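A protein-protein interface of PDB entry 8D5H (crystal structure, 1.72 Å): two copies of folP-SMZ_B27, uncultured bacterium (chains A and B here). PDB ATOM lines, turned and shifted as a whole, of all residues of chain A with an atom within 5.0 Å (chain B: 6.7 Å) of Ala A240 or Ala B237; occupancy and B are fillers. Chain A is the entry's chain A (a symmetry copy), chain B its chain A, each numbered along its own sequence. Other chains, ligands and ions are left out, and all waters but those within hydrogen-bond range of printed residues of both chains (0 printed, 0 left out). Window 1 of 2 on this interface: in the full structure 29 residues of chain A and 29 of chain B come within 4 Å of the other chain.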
ATOM      1  N   THR A 235       2.010  15.845 -10.823  1.00  0.00           N
ATOM      2  CA  THR A 235       2.905  16.151 -11.945  1.00  0.00           C
ATOM      3  C   THR A 235       3.924  15.021 -12.145  1.00  0.00           C
ATOM      4  O   THR A 235       4.249  14.640 -13.279  1.00  0.00           O
ATOM      5  CB  THR A 235       3.637  17.473 -11.702  1.00  0.00           C
ATOM      6  OG1 THR A 235       2.655  18.507 -11.574  1.00  0.00           O
ATOM      7  CG2 THR A 235       4.439  17.854 -12.941  1.00  0.00           C
ATOM      8  N   ILE A 236       4.436  14.487 -11.056  1.00  0.00           N
ATOM      9  CA  ILE A 236       5.355  13.353 -11.155  1.00  0.00           C
ATOM     10  C   ILE A 236       4.663  12.164 -11.815  1.00  0.00           C
ATOM     11  O   ILE A 236       5.212  11.524 -12.719  1.00  0.00           O
ATOM     12  CB  ILE A 236       5.912  13.001  -9.773  1.00  0.00           C
ATOM     13  CG1 ILE A 236       6.856  14.132  -9.272  1.00  0.00           C
ATOM     14  CG2 ILE A 236       6.652  11.641  -9.846  1.00  0.00           C
ATOM     15  CD1 ILE A 236       7.173  13.967  -7.729  1.00  0.00           C
ATOM     16  N   ALA A 237       3.457  11.829 -11.355  1.00  0.00           N
ATOM     17  CA  ALA A 237       2.747  10.675 -11.895  1.00  0.00           C
ATOM     18  C   ALA A 237       2.421  10.876 -13.373  1.00  0.00           C
ATOM     19  O   ALA A 237       2.623   9.981 -14.194  1.00  0.00           O
ATOM     20  CB  ALA A 237       1.467  10.427 -11.112  1.00  0.00           C
ATOM     21  N   ALA A 238       1.935  12.064 -13.725  1.00  0.00           N
ATOM     22  CA  ALA A 238       1.561  12.314 -15.116  1.00  0.00           C
ATOM     23  C   ALA A 238       2.791  12.306 -16.009  1.00  0.00           C
ATOM     24  O   ALA A 238       2.745  11.760 -17.132  1.00  0.00           O
ATOM     25  CB  ALA A 238       0.835  13.668 -15.224  1.00  0.00           C
ATOM     26  N   SER A 239       3.896  12.908 -15.539  1.00  0.00           N
ATOM     27  CA  SER A 239       5.111  12.964 -16.363  1.00  0.00           C
ATOM     28  C   SER A 239       5.708  11.581 -16.520  1.00  0.00           C
ATOM     29  O   SER A 239       6.164  11.220 -17.616  1.00  0.00           O
ATOM     30  CB  SER A 239       6.145  13.904 -15.717  1.00  0.00           C
ATOM     31  OG  SER A 239       5.614  15.241 -15.670  1.00  0.00           O
ATOM     32  N   ALA A 240       5.661  10.782 -15.447  1.00  0.00           N
ATOM     33  CA  ALA A 240       6.146   9.396 -15.543  1.00  0.00           C
ATOM     34  C   ALA A 240       5.319   8.587 -16.545  1.00  0.00           C
ATOM     35  O   ALA A 240       5.869   7.833 -17.348  1.00  0.00           O
ATOM     36  CB  ALA A 240       6.129   8.736 -14.152  1.00  0.00           C
ATOM     37  N   ILE A 241       3.990   8.688 -16.481  1.00  0.00           N
ATOM     38  CA  ILE A 241       3.167   7.917 -17.408  1.00  0.00           C
ATOM     39  C   ILE A 241       3.365   8.447 -18.832  1.00  0.00           C
ATOM     40  O   ILE A 241       3.300   7.677 -19.790  1.00  0.00           O
ATOM     41  CB  ILE A 241       1.698   7.969 -16.949  1.00  0.00           C
ATOM     42  CG1 ILE A 241       1.596   7.151 -15.620  1.00  0.00           C
ATOM     43  CG2 ILE A 241       0.713   7.436 -17.990  1.00  0.00           C
ATOM     44  CD1 ILE A 241       0.272   7.336 -14.816  1.00  0.00           C
ATOM     45  N   ALA A 242       3.575   9.763 -18.986  1.00  0.00           N
ATOM     46  CA  ALA A 242       3.850  10.302 -20.328  1.00  0.00           C
ATOM     47  C   ALA A 242       5.099   9.643 -20.925  1.00  0.00           C
ATOM     48  O   ALA A 242       5.111   9.215 -22.099  1.00  0.00           O
ATOM     49  CB  ALA A 242       4.038  11.829 -20.288  1.00  0.00           C
ATOM     50  N   VAL A 243       6.161   9.559 -20.139  1.00  0.00           N
ATOM     51  CA  VAL A 243       7.368   8.850 -20.591  1.00  0.00           C
ATOM     52  C   VAL A 243       7.075   7.381 -20.854  1.00  0.00           C
ATOM     53  O   VAL A 243       7.530   6.826 -21.860  1.00  0.00           O
ATOM     54  CB  VAL A 243       8.518   9.024 -19.568  1.00  0.00           C
ATOM     55  CG1 VAL A 243       9.731   8.116 -19.853  1.00  0.00           C
ATOM     56  CG2 VAL A 243       8.973  10.476 -19.536  1.00  0.00           C
ATOM     57  N   LEU A 244       6.387   6.699 -19.935  1.00  0.00           N
ATOM     58  CA  LEU A 244       6.007   5.317 -20.192  1.00  0.00           C
ATOM     59  C   LEU A 244       5.337   5.156 -21.566  1.00  0.00           C
ATOM     60  O   LEU A 244       5.520   4.127 -22.258  1.00  0.00           O
ATOM     61  CB  LEU A 244       5.059   4.827 -19.085  1.00  0.00           C
ATOM     62  CG  LEU A 244       4.848   3.305 -19.061  1.00  0.00           C
ATOM     63  CD1 LEU A 244       6.025   2.615 -18.436  1.00  0.00           C
ATOM     64  CD2 LEU A 244       3.595   3.027 -18.221  1.00  0.00           C
ATOM     65  N   GLY A 261      11.367  10.799 -11.142  1.00  0.00           N
ATOM     66  CA  GLY A 261      10.177   9.992 -11.397  1.00  0.00           C
ATOM     67  C   GLY A 261      10.194   9.439 -12.818  1.00  0.00           C
ATOM     68  O   GLY A 261       9.822   8.279 -13.063  1.00  0.00           O
ATOM     69  N   CYS A 262      10.652  10.254 -13.776  1.00  0.00           N
ATOM     70  CA  CYS A 262      10.696   9.754 -15.160  1.00  0.00           C
ATOM     71  C   CYS A 262      11.732   8.657 -15.343  1.00  0.00           C
ATOM     72  O   CYS A 262      11.537   7.810 -16.231  1.00  0.00           O
ATOM     73  CB  CYS A 262      10.979  10.909 -16.138  1.00  0.00           C
ATOM     74  SG  CYS A 262       9.512  11.984 -16.268  1.00  0.00           S
ATOM     75  N   ILE A 264      12.267   6.295 -13.430  1.00  0.00           N
ATOM     76  CA  ILE A 264      11.584   5.053 -13.051  1.00  0.00           C
ATOM     77  C   ILE A 264      10.706   4.553 -14.199  1.00  0.00           C
ATOM     78  O   ILE A 264      10.697   3.356 -14.512  1.00  0.00           O
ATOM     79  CB  ILE A 264      10.761   5.263 -11.740  1.00  0.00           C
ATOM     80  CG1 ILE A 264      11.701   5.573 -10.558  1.00  0.00           C
ATOM     81  CG2 ILE A 264       9.885   3.992 -11.412  1.00  0.00           C
ATOM     82  CD1 ILE A 264      12.948   4.661 -10.427  1.00  0.00           C
ATOM     83  N   ALA A 265      10.017   5.459 -14.889  1.00  0.00           N
ATOM     84  CA  ALA A 265       9.267   5.099 -16.079  1.00  0.00           C
ATOM     85  C   ALA A 265      10.182   4.485 -17.144  1.00  0.00           C
ATOM     86  O   ALA A 265       9.849   3.459 -17.755  1.00  0.00           O
ATOM     87  CB  ALA A 265       8.550   6.363 -16.620  1.00  0.00           C
ATOM     88  N   LEU B 220      14.198   1.364  -6.163  1.00  0.00           N
ATOM     89  CA  LEU B 220      14.001   2.741  -6.631  1.00  0.00           C
ATOM     90  C   LEU B 220      15.228   3.627  -6.472  1.00  0.00           C
ATOM     91  O   LEU B 220      15.144   4.839  -6.723  1.00  0.00           O
ATOM     92  CB  LEU B 220      12.827   3.353  -5.868  1.00  0.00           C
ATOM     93  CG  LEU B 220      11.529   2.587  -6.141  1.00  0.00           C
ATOM     94  CD1 LEU B 220      10.461   3.027  -5.156  1.00  0.00           C
ATOM     95  CD2 LEU B 220      11.037   2.770  -7.616  1.00  0.00           C
ATOM     96  N   LEU B 232      11.012   9.449  -2.788  1.00  0.00           N
ATOM     97  CA  LEU B 232       9.577   9.714  -2.898  1.00  0.00           C
ATOM     98  C   LEU B 232       9.151   9.936  -4.344  1.00  0.00           C
ATOM     99  O   LEU B 232       8.140   9.342  -4.762  1.00  0.00           O
ATOM    100  CB  LEU B 232       9.174  10.870  -1.975  1.00  0.00           C
ATOM    101  CG  LEU B 232       7.674  11.202  -2.042  1.00  0.00           C
ATOM    102  CD1 LEU B 232       6.811   9.987  -1.761  1.00  0.00           C
ATOM    103  CD2 LEU B 232       7.356  12.385  -1.086  1.00  0.00           C
ATOM    104  N   PRO B 233       9.858  10.719  -5.164  1.00  0.00           N
ATOM    105  CA  PRO B 233       9.408  10.819  -6.562  1.00  0.00           C
ATOM    106  C   PRO B 233       9.341   9.459  -7.244  1.00  0.00           C
ATOM    107  O   PRO B 233       8.363   9.163  -7.947  1.00  0.00           O
ATOM    108  CB  PRO B 233      10.439  11.771  -7.200  1.00  0.00           C
ATOM    109  CG  PRO B 233      10.906  12.671  -6.009  1.00  0.00           C
ATOM    110  CD  PRO B 233      10.975  11.655  -4.862  1.00  0.00           C
ATOM    111  N   GLY B 234      10.322   8.595  -7.002  1.00  0.00           N
ATOM    112  CA  GLY B 234      10.288   7.290  -7.655  1.00  0.00           C
ATOM    113  C   GLY B 234       9.172   6.415  -7.116  1.00  0.00           C
ATOM    114  O   GLY B 234       8.577   5.641  -7.870  1.00  0.00           O
ATOM    115  N   THR B 235       8.869   6.533  -5.814  1.00  0.00           N
ATOM    116  CA  THR B 235       7.753   5.765  -5.248  1.00  0.00           C
ATOM    117  C   THR B 235       6.419   6.235  -5.844  1.00  0.00           C
ATOM    118  O   THR B 235       5.526   5.428  -6.142  1.00  0.00           O
ATOM    119  CB  THR B 235       7.720   5.909  -3.725  1.00  0.00           C
ATOM    120  OG1 THR B 235       8.959   5.411  -3.206  1.00  0.00           O
ATOM    121  CG2 THR B 235       6.660   4.984  -3.142  1.00  0.00           C
ATOM    122  N   ILE B 236       6.271   7.533  -6.013  1.00  0.00           N
ATOM    123  CA  ILE B 236       5.062   8.058  -6.646  1.00  0.00           C
ATOM    124  C   ILE B 236       4.929   7.521  -8.068  1.00  0.00           C
ATOM    125  O   ILE B 236       3.857   7.066  -8.484  1.00  0.00           O
ATOM    126  CB  ILE B 236       5.068   9.589  -6.608  1.00  0.00           C
ATOM    127  CG1 ILE B 236       4.902  10.089  -5.144  1.00  0.00           C
ATOM    128  CG2 ILE B 236       3.938  10.133  -7.519  1.00  0.00           C
ATOM    129  CD1 ILE B 236       5.243  11.631  -5.026  1.00  0.00           C
ATOM    130  N   ALA B 237       6.009   7.590  -8.848  1.00  0.00           N
ATOM    131  CA  ALA B 237       5.954   7.144 -10.236  1.00  0.00           C
ATOM    132  C   ALA B 237       5.662   5.648 -10.319  1.00  0.00           C
ATOM    133  O   ALA B 237       4.823   5.209 -11.106  1.00  0.00           O
ATOM    134  CB  ALA B 237       7.265   7.455 -10.943  1.00  0.00           C
ATOM    135  N   ALA B 238       6.337   4.857  -9.489  1.00  0.00           N
ATOM    136  CA  ALA B 238       6.139   3.409  -9.542  1.00  0.00           C
ATOM    137  C   ALA B 238       4.733   3.047  -9.096  1.00  0.00           C
ATOM    138  O   ALA B 238       4.093   2.159  -9.700  1.00  0.00           O
ATOM    139  CB  ALA B 238       7.178   2.709  -8.645  1.00  0.00           C
ATOM    140  N   SER B 239       4.231   3.710  -8.040  1.00  0.00           N
ATOM    141  CA  SER B 239       2.889   3.388  -7.537  1.00  0.00           C
ATOM    142  C   SER B 239       1.834   3.811  -8.537  1.00  0.00           C
ATOM    143  O   SER B 239       0.856   3.079  -8.758  1.00  0.00           O
ATOM    144  CB  SER B 239       2.644   4.098  -6.194  1.00  0.00           C
ATOM    145  OG  SER B 239       3.580   3.612  -5.216  1.00  0.00           O
ATOM    146  N   ALA B 240       2.049   4.961  -9.186  1.00  0.00           N
ATOM    147  CA  ALA B 240       1.111   5.400 -10.233  1.00  0.00           C
ATOM    148  C   ALA B 240       1.079   4.409 -11.399  1.00  0.00           C
ATOM    149  O   ALA B 240       0.009   4.075 -11.908  1.00  0.00           O
ATOM    150  CB  ALA B 240       1.488   6.812 -10.717  1.00  0.00           C
ATOM    151  N   ILE B 241       2.246   3.968 -11.874  1.00  0.00           N
ATOM    152  CA  ILE B 241       2.255   3.037 -12.997  1.00  0.00           C
ATOM    153  C   ILE B 241       1.669   1.692 -12.555  1.00  0.00           C
ATOM    154  O   ILE B 241       1.037   1.003 -13.356  1.00  0.00           O
ATOM    155  CB  ILE B 241       3.690   2.913 -13.544  1.00  0.00           C
ATOM    156  CG1 ILE B 241       4.054   4.279 -14.211  1.00  0.00           C
ATOM    157  CG2 ILE B 241       3.871   1.761 -14.533  1.00  0.00           C
ATOM    158  CD1 ILE B 241       5.564   4.484 -14.546  1.00  0.00           C
ATOM    159  N   ALA B 242       1.897   1.295 -11.295  1.00  0.00           N
ATOM    160  CA  ALA B 242       1.285   0.048 -10.805  1.00  0.00           C
ATOM    161  C   ALA B 242      -0.243   0.124 -10.911  1.00  0.00           C
ATOM    162  O   ALA B 242      -0.910  -0.818 -11.388  1.00  0.00           O
ATOM    163  CB  ALA B 242       1.690  -0.236  -9.347  1.00  0.00           C
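CG2 of Ile A236 touches O of Pro B233, at 3.6 Å. Ile B236 touches Ile A236 (CG2 to CG2, 3.9 Å). CB of Ala B240 touches CB of Ala A237 (3.6 Å). CB of Ala A240 touches CB of Ala B237, at 3.6 Å. Leu A244 touches Ile B241. Gly A261 touches Pro B233 (CA to O, 3.99 Å). Gly A261 touches Ala B237 (O to CB, 3.4 Å). Ile A264 touches Leu B220. Ile A264 touches Gly B234 (CG1 to CA, 3.7 Å).
Of chain B, only Ala B237 (3.6 Å) comes within 4 Å of Ala A240. Of the printed residues of chain B, Gly A261 touches Pro B233 (3.99 Å) and Ala B237 (3.4 Å). Of the printed residues of chain A, Ile B236 touches Ile A236. Ala B237 touches just these residues of chain A: Ala A240 and Gly A261. Ala B238 touches none of the printed residues of chain A. Ala B242 touches none of the printed residues of chain A. The nearest residue of chain B that does not touch Ala A240 is Ile B241 (4.3 Å). The nearest printed residue of chain B that does not touch Gly A261 is Gly B234 (4.6 Å).
Hydrophobic or aromatic side chains of chain B within 4 Å of the printed part of chain A: Leu B220, Pro B233, Ile B236, Ala B237, Ala B240 and Ile B241. Printed residues of chain A that touch a printed residue of chain B: Ile A236, Ala A237, Ala A240, Leu A244, Gly A261 and Ile A264. Hydrophobic or aromatic side chains of chain A within 4 Å of the printed part of chain B: Ile A236, Ala A237, Ala A240, Leu A244 and Ile A264. Among the printed residues, no Asp or Glu carboxylate lies within 4 Å of a Lys or Arg side-chain nitrogen of the other chain.
Ile B236 touches its own counterpart, Ile A236. Ala A237 touches Ala B240, and with the chains exchanged Ala A240 touches Ala B237. 8 positions are printed for both chains. Of the 9 pairs that touch across the chains among the printed residues, 3 have their exchanged pair printed and touching as well.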
